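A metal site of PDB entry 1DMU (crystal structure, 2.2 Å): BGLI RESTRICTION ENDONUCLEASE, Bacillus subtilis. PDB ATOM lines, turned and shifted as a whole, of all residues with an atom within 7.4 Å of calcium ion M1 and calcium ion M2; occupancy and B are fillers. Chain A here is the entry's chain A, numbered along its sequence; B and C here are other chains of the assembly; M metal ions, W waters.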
ATOM      1  N   ILE A  83       1.317   5.890   9.033  1.00  0.00           N
ATOM      2  CA  ILE A  83       1.766   4.790   9.886  1.00  0.00           C
ATOM      3  C   ILE A  83       3.212   4.308   9.696  1.00  0.00           C
ATOM      4  O   ILE A  83       3.963   4.223  10.651  1.00  0.00           O
ATOM      5  CB  ILE A  83       0.843   3.554   9.714  1.00  0.00           C
ATOM      6  CG1 ILE A  83      -0.620   3.949   9.861  1.00  0.00           C
ATOM      7  CG2 ILE A  83       1.143   2.499  10.806  1.00  0.00           C
ATOM      8  CD1 ILE A  83      -1.598   2.878   9.315  1.00  0.00           C
ATOM      9  N   GLU A  87       7.066   4.322  11.790  1.00  0.00           N
ATOM     10  CA  GLU A  87       7.557   2.993  12.125  1.00  0.00           C
ATOM     11  C   GLU A  87       9.002   2.782  11.708  1.00  0.00           C
ATOM     12  O   GLU A  87       9.783   2.184  12.441  1.00  0.00           O
ATOM     13  CB  GLU A  87       6.710   1.914  11.447  1.00  0.00           C
ATOM     14  CG  GLU A  87       5.352   1.726  12.073  1.00  0.00           C
ATOM     15  CD  GLU A  87       4.559   0.603  11.424  1.00  0.00           C
ATOM     16  OE1 GLU A  87       4.756   0.337  10.226  1.00  0.00           O
ATOM     17  OE2 GLU A  87       3.724  -0.009  12.122  1.00  0.00           O
ATOM     18  N   GLY A 114       3.733 -10.083  19.307  1.00  0.00           N
ATOM     19  CA  GLY A 114       4.327  -9.002  20.056  1.00  0.00           C
ATOM     20  C   GLY A 114       4.305  -7.696  19.321  1.00  0.00           C
ATOM     21  O   GLY A 114       3.746  -7.599  18.227  1.00  0.00           O
ATOM     22  N   PRO A 115       4.961  -6.657  19.901  1.00  0.00           N
ATOM     23  CA  PRO A 115       5.055  -5.300  19.371  1.00  0.00           C
ATOM     24  C   PRO A 115       5.958  -5.118  18.140  1.00  0.00           C
ATOM     25  O   PRO A 115       6.632  -6.048  17.695  1.00  0.00           O
ATOM     26  CB  PRO A 115       5.553  -4.504  20.575  1.00  0.00           C
ATOM     27  CG  PRO A 115       6.407  -5.480  21.314  1.00  0.00           C
ATOM     28  CD  PRO A 115       5.709  -6.793  21.166  1.00  0.00           C
ATOM     29  N   ASP A 116       5.957  -3.909  17.583  1.00  0.00           N
ATOM     30  CA  ASP A 116       6.755  -3.546  16.414  1.00  0.00           C
ATOM     31  C   ASP A 116       8.194  -4.001  16.538  1.00  0.00           C
ATOM     32  O   ASP A 116       8.708  -4.687  15.656  1.00  0.00           O
ATOM     33  CB  ASP A 116       6.746  -2.033  16.204  1.00  0.00           C
ATOM     34  CG  ASP A 116       5.404  -1.517  15.754  1.00  0.00           C
ATOM     35  OD1 ASP A 116       4.596  -2.323  15.267  1.00  0.00           O
ATOM     36  OD2 ASP A 116       5.165  -0.293  15.901  1.00  0.00           O
ATOM     37  N   GLU A 117       8.857  -3.605  17.624  1.00  0.00           N
ATOM     38  CA  GLU A 117      10.264  -3.971  17.831  1.00  0.00           C
ATOM     39  C   GLU A 117      10.427  -4.838  19.075  1.00  0.00           C
ATOM     40  O   GLU A 117       9.825  -4.567  20.126  1.00  0.00           O
ATOM     41  CB  GLU A 117      11.114  -2.694  17.969  1.00  0.00           C
ATOM     42  CG  GLU A 117      10.978  -1.702  16.789  1.00  0.00           C
ATOM     43  CD  GLU A 117      11.575  -2.226  15.470  1.00  0.00           C
ATOM     44  OE1 GLU A 117      12.518  -3.047  15.490  1.00  0.00           O
ATOM     45  OE2 GLU A 117      11.091  -1.817  14.402  1.00  0.00           O
ATOM     46  N   VAL A 141       9.038  -2.581  22.171  1.00  0.00           N
ATOM     47  CA  VAL A 141       8.768  -1.200  21.776  1.00  0.00           C
ATOM     48  C   VAL A 141       7.788  -1.124  20.633  1.00  0.00           C
ATOM     49  O   VAL A 141       7.934  -1.785  19.606  1.00  0.00           O
ATOM     50  CB  VAL A 141      10.097  -0.465  21.343  1.00  0.00           C
ATOM     51  CG1 VAL A 141       9.903   1.047  21.378  1.00  0.00           C
ATOM     52  CG2 VAL A 141      11.263  -0.875  22.258  1.00  0.00           C
ATOM     53  N   ASP A 142       6.765  -0.307  20.801  1.00  0.00           N
ATOM     54  CA  ASP A 142       5.802  -0.166  19.725  1.00  0.00           C
ATOM     55  C   ASP A 142       5.621   1.328  19.407  1.00  0.00           C
ATOM     56  O   ASP A 142       5.517   2.153  20.294  1.00  0.00           O
ATOM     57  CB  ASP A 142       4.483  -0.843  20.109  1.00  0.00           C
ATOM     58  CG  ASP A 142       3.671  -1.246  18.901  1.00  0.00           C
ATOM     59  OD1 ASP A 142       2.866  -0.421  18.452  1.00  0.00           O
ATOM     60  OD2 ASP A 142       3.834  -2.385  18.394  1.00  0.00           O
ATOM     61  N   ILE A 143       5.618   1.632  18.101  1.00  0.00           N
ATOM     62  CA  ILE A 143       5.460   2.981  17.593  1.00  0.00           C
ATOM     63  C   ILE A 143       3.977   3.284  17.358  1.00  0.00           C
ATOM     64  O   ILE A 143       3.287   2.529  16.653  1.00  0.00           O
ATOM     65  CB  ILE A 143       6.195   3.140  16.240  1.00  0.00           C
ATOM     66  CG1 ILE A 143       7.701   3.123  16.482  1.00  0.00           C
ATOM     67  CG2 ILE A 143       5.809   4.445  15.571  1.00  0.00           C
ATOM     68  CD1 ILE A 143       8.237   4.448  17.007  1.00  0.00           C
ATOM     69  N   LYS A 144       3.488   4.377  17.925  1.00  0.00           N
ATOM     70  CA  LYS A 144       2.083   4.769  17.787  1.00  0.00           C
ATOM     71  C   LYS A 144       2.050   6.224  17.290  1.00  0.00           C
ATOM     72  O   LYS A 144       2.200   7.145  18.064  1.00  0.00           O
ATOM     73  CB  LYS A 144       1.346   4.673  19.148  1.00  0.00           C
ATOM     74  CG  LYS A 144       1.476   3.341  19.929  1.00  0.00           C
ATOM     75  CD  LYS A 144       0.672   2.265  19.245  1.00  0.00           C
ATOM     76  CE  LYS A 144       0.560   0.994  20.049  1.00  0.00           C
ATOM     77  NZ  LYS A 144      -0.058  -0.020  19.161  1.00  0.00           N
ATOM     78  N   SER A 145       1.837   6.414  15.993  1.00  0.00           N
ATOM     79  CA  SER A 145       1.790   7.745  15.411  1.00  0.00           C
ATOM     80  C   SER A 145       0.385   8.334  15.413  1.00  0.00           C
ATOM     81  O   SER A 145      -0.594   7.619  15.228  1.00  0.00           O
ATOM     82  CB  SER A 145       2.317   7.708  13.972  1.00  0.00           C
ATOM     83  OG  SER A 145       3.328   6.739  13.785  1.00  0.00           O
ATOM     84  N   GLN A 161       0.592  -6.494  23.379  1.00  0.00           N
ATOM     85  CA  GLN A 161       1.472  -5.389  23.717  1.00  0.00           C
ATOM     86  C   GLN A 161       1.516  -5.088  25.230  1.00  0.00           C
ATOM     87  O   GLN A 161       2.151  -4.131  25.679  1.00  0.00           O
ATOM     88  CB  GLN A 161       1.052  -4.142  22.905  1.00  0.00           C
ATOM     89  CG  GLN A 161       1.508  -4.223  21.447  1.00  0.00           C
ATOM     90  CD  GLN A 161       0.769  -3.264  20.513  1.00  0.00           C
ATOM     91  OE1 GLN A 161       0.248  -2.241  20.942  1.00  0.00           O
ATOM     92  NE2 GLN A 161       0.751  -3.592  19.202  1.00  0.00           N
ATOM     93  N   PHE A 213       6.695   2.711  24.704  1.00  0.00           N
ATOM     94  CA  PHE A 213       5.895   3.166  23.575  1.00  0.00           C
ATOM     95  C   PHE A 213       6.469   4.470  23.068  1.00  0.00           C
ATOM     96  O   PHE A 213       6.767   5.369  23.850  1.00  0.00           O
ATOM     97  CB  PHE A 213       4.440   3.286  24.014  1.00  0.00           C
ATOM     98  CG  PHE A 213       3.841   1.959  24.307  1.00  0.00           C
ATOM     99  CD1 PHE A 213       3.791   1.483  25.613  1.00  0.00           C
ATOM    100  CD2 PHE A 213       3.474   1.114  23.264  1.00  0.00           C
ATOM    101  CE1 PHE A 213       3.415   0.177  25.865  1.00  0.00           C
ATOM    102  CE2 PHE A 213       3.091  -0.202  23.510  1.00  0.00           C
ATOM    103  CZ  PHE A 213       3.070  -0.669  24.812  1.00  0.00           C
ATOM    104  N   ILE A 214       6.665   4.526  21.756  1.00  0.00           N
ATOM    105  CA  ILE A 214       7.184   5.723  21.101  1.00  0.00           C
ATOM    106  C   ILE A 214       6.036   6.294  20.265  1.00  0.00           C
ATOM    107  O   ILE A 214       5.504   5.651  19.354  1.00  0.00           O
ATOM    108  CB  ILE A 214       8.374   5.405  20.198  1.00  0.00           C
ATOM    109  CG1 ILE A 214       9.487   4.784  21.050  1.00  0.00           C
ATOM    110  CG2 ILE A 214       8.830   6.663  19.498  1.00  0.00           C
ATOM    111  CD1 ILE A 214      10.769   4.641  20.311  1.00  0.00           C
ATOM    112  P    DT B  10      -1.759  -8.040  16.720  1.00  0.00           P
ATOM    113  OP1  DT B  10      -0.586  -8.315  17.590  1.00  0.00           O
ATOM    114  OP2  DT B  10      -3.103  -7.864  17.323  1.00  0.00           O
ATOM    115  O5'  DT B  10      -1.489  -6.748  15.835  1.00  0.00           O
ATOM    116  C5'  DT B  10      -0.618  -6.832  14.727  1.00  0.00           C
ATOM    117  C4'  DT B  10      -0.634  -5.539  13.975  1.00  0.00           C
ATOM    118  O4'  DT B  10      -1.754  -5.525  13.064  1.00  0.00           O
ATOM    119  C3'  DT B  10      -0.778  -4.312  14.872  1.00  0.00           C
ATOM    120  O3'  DT B  10       0.173  -3.322  14.505  1.00  0.00           O
ATOM    121  C2'  DT B  10      -2.202  -3.830  14.597  1.00  0.00           C
ATOM    122  C1'  DT B  10      -2.401  -4.270  13.154  1.00  0.00           C
ATOM    123  N1   DT B  10      -3.808  -4.440  12.734  1.00  0.00           N
ATOM    124  C2   DT B  10      -4.196  -3.876  11.530  1.00  0.00           C
ATOM    125  O2   DT B  10      -3.429  -3.271  10.809  1.00  0.00           O
ATOM    126  N3   DT B  10      -5.532  -4.038  11.211  1.00  0.00           N
ATOM    127  C4   DT B  10      -6.491  -4.705  11.957  1.00  0.00           C
ATOM    128  O4   DT B  10      -7.637  -4.777  11.548  1.00  0.00           O
ATOM    129  C5   DT B  10      -6.016  -5.275  13.202  1.00  0.00           C
ATOM    130  C7   DT B  10      -6.979  -6.014  14.080  1.00  0.00           C
ATOM    131  C6   DT B  10      -4.720  -5.124  13.522  1.00  0.00           C
ATOM    132  P    DA B  11       0.346  -2.025  15.408  1.00  0.00           P
ATOM    133  OP1  DA B  11       1.772  -1.614  15.277  1.00  0.00           O
ATOM    134  OP2  DA B  11      -0.242  -2.205  16.768  1.00  0.00           O
ATOM    135  O5'  DA B  11      -0.555  -0.981  14.640  1.00  0.00           O
ATOM    136  C5'  DA B  11      -0.412  -0.824  13.248  1.00  0.00           C
ATOM    137  C4'  DA B  11      -1.321   0.245  12.748  1.00  0.00           C
ATOM    138  O4'  DA B  11      -2.626  -0.287  12.389  1.00  0.00           O
ATOM    139  C3'  DA B  11      -1.530   1.344  13.766  1.00  0.00           C
ATOM    140  O3'  DA B  11      -1.065   2.619  13.309  1.00  0.00           O
ATOM    141  C2'  DA B  11      -3.039   1.346  14.008  1.00  0.00           C
ATOM    142  C1'  DA B  11      -3.645   0.598  12.836  1.00  0.00           C
ATOM    143  N9   DA B  11      -4.835  -0.191  13.194  1.00  0.00           N
ATOM    144  C8   DA B  11      -4.978  -1.080  14.233  1.00  0.00           C
ATOM    145  N7   DA B  11      -6.167  -1.613  14.323  1.00  0.00           N
ATOM    146  C5   DA B  11      -6.868  -1.043  13.273  1.00  0.00           C
ATOM    147  C6   DA B  11      -8.193  -1.182  12.833  1.00  0.00           C
ATOM    148  N6   DA B  11      -9.096  -1.987  13.418  1.00  0.00           N
ATOM    149  N1   DA B  11      -8.578  -0.481  11.751  1.00  0.00           N
ATOM    150  C2   DA B  11      -7.684   0.327  11.154  1.00  0.00           C
ATOM    151  N3   DA B  11      -6.415   0.556  11.486  1.00  0.00           N
ATOM    152  C4   DA B  11      -6.055  -0.172  12.563  1.00  0.00           C
ATOM    153  P    DG B  12      -0.711   3.753  14.378  1.00  0.00           P
ATOM    154  OP1  DG B  12       0.545   4.420  14.004  1.00  0.00           O
ATOM    155  OP2  DG B  12      -0.853   3.188  15.753  1.00  0.00           O
ATOM    156  O5'  DG B  12      -1.866   4.831  14.166  1.00  0.00           O
ATOM    157  C5'  DG B  12      -2.161   5.328  12.862  1.00  0.00           C
ATOM    158  C4'  DG B  12      -3.502   6.040  12.852  1.00  0.00           C
ATOM    159  O4'  DG B  12      -4.576   5.077  12.939  1.00  0.00           O
ATOM    160  C3'  DG B  12      -3.720   7.018  14.011  1.00  0.00           C
ATOM    161  O3'  DG B  12      -4.564   8.068  13.566  1.00  0.00           O
ATOM    162  C2'  DG B  12      -4.542   6.197  14.979  1.00  0.00           C
ATOM    163  C1'  DG B  12      -5.438   5.469  13.994  1.00  0.00           C
ATOM    164  N9   DG B  12      -6.154   4.295  14.481  1.00  0.00           N
ATOM    165  C8   DG B  12      -5.762   3.423  15.470  1.00  0.00           C
ATOM    166  N7   DG B  12      -6.642   2.492  15.697  1.00  0.00           N
ATOM    167  C5   DG B  12      -7.665   2.759  14.807  1.00  0.00           C
ATOM    168  C6   DG B  12      -8.904   2.091  14.592  1.00  0.00           C
ATOM    169  O6   DG B  12      -9.336   1.089  15.162  1.00  0.00           O
ATOM    170  N1   DG B  12      -9.652   2.692  13.595  1.00  0.00           N
ATOM    171  C2   DG B  12      -9.262   3.803  12.883  1.00  0.00           C
ATOM    172  N2   DG B  12     -10.135   4.223  11.941  1.00  0.00           N
ATOM    173  N3   DG B  12      -8.125   4.435  13.069  1.00  0.00           N
ATOM    174  C4   DG B  12      -7.378   3.865  14.046  1.00  0.00           C
ATOM    175  N   GLU C  84       5.893 -13.853  12.080  1.00  0.00           N
ATOM    176  CA  GLU C  84       6.769 -12.931  12.798  1.00  0.00           C
ATOM    177  C   GLU C  84       8.110 -13.502  13.245  1.00  0.00           C
ATOM    178  O   GLU C  84       9.066 -12.748  13.456  1.00  0.00           O
ATOM    179  CB  GLU C  84       6.025 -12.314  13.999  1.00  0.00           C
ATOM    180  CG  GLU C  84       4.633 -11.761  13.661  1.00  0.00           C
ATOM    181  CD  GLU C  84       4.060 -10.893  14.780  1.00  0.00           C
ATOM    182  OE1 GLU C  84       4.761 -10.689  15.790  1.00  0.00           O
ATOM    183  OE2 GLU C  84       2.911 -10.423  14.643  1.00  0.00           O
HETATM  184 CA    CA M   1       2.955   0.250  16.084  1.00  0.00          CA
HETATM  185 CA    CA M   2       2.974  -3.485  14.097  1.00  0.00          CA
HETATM  186  O   HOH W   1       5.017  -4.170  12.977  1.00  0.00           O
HETATM  187  O   HOH W   2       2.473  -6.047  13.885  1.00  0.00           O
HETATM  188  O   HOH W   3       2.778  -4.092  16.584  1.00  0.00           O
HETATM  189  O   HOH W   4       1.753  -3.331  11.990  1.00  0.00           O
HETATM  190  O   HOH W   5       0.265   0.990  16.527  1.00  0.00           O
HETATM  191  O   HOH W   6       2.614   1.406  13.942  1.00  0.00           O
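Calcium ion M2 is bound by OD1 of Asp 116 (2.3 Å), water W1 (2.4 Å), water W4 (2.4 Å), OP1 of DA 11 of chain B (2.5 Å), water W3 (2.6 Å), water W2 (2.6 Å) and O3' of DT 10 of chain B (2.8 Å).
Water W5 lies within hydrogen-bond range of OP2 of DG 12 of chain B (2.6 Å), NZ of Lys 144 (2.8 Å) and O5' of DA 11 of chain B (2.8 Å).
Water W3 lies within hydrogen-bond range of the side-chain carboxylate of Asp 142, the backbone NH of Asp 116 and the side-chain amide nitrogen of Gln 161.
Within 4 Å of calcium ion M1: Asp 116, Asp 142, Ile 143 and DA 11 of chain B.
The nearest printed residue that does not touch calcium ion M1 is Glu 87 (4.04 Å).
OP2 of DA 11 of chain B is in salt-bridge range of the side-chain amino group (NZ) of Lys 144, 3.2 Å away.
The side-chain amide nitrogen (NE2) of Gln 161 lies within hydrogen-bond range of OP2 of DA 11 of chain B, at 3.0 Å.
NZ of Lys 144 lies close to OD1 of Asp 142.
The side-chain carboxylate (OD2) of Asp 142 lies within hydrogen-bond range of the side-chain amide nitrogen (NE2) of Gln 161, 3.4 Å away.
The backbone carbonyl oxygen (O) of Asp 142 sits at hydrogen-bond distance from the backbone NH (N) of Ile 214 (3.0 Å).
Calcium ion M1 is bound by the side-chain carboxylate (OD2) of Asp 116 (2.3 Å), OP1 of DA 11 of chain B (2.4 Å), the backbone carbonyl oxygen (O) of Ile 143 (2.4 Å), water W6 (2.5 Å), the side-chain carboxylate (OD1) of Asp 142 (2.5 Å) and water W5 (2.8 Å).
Calcium ion M1 has six donor atoms within binding distance.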
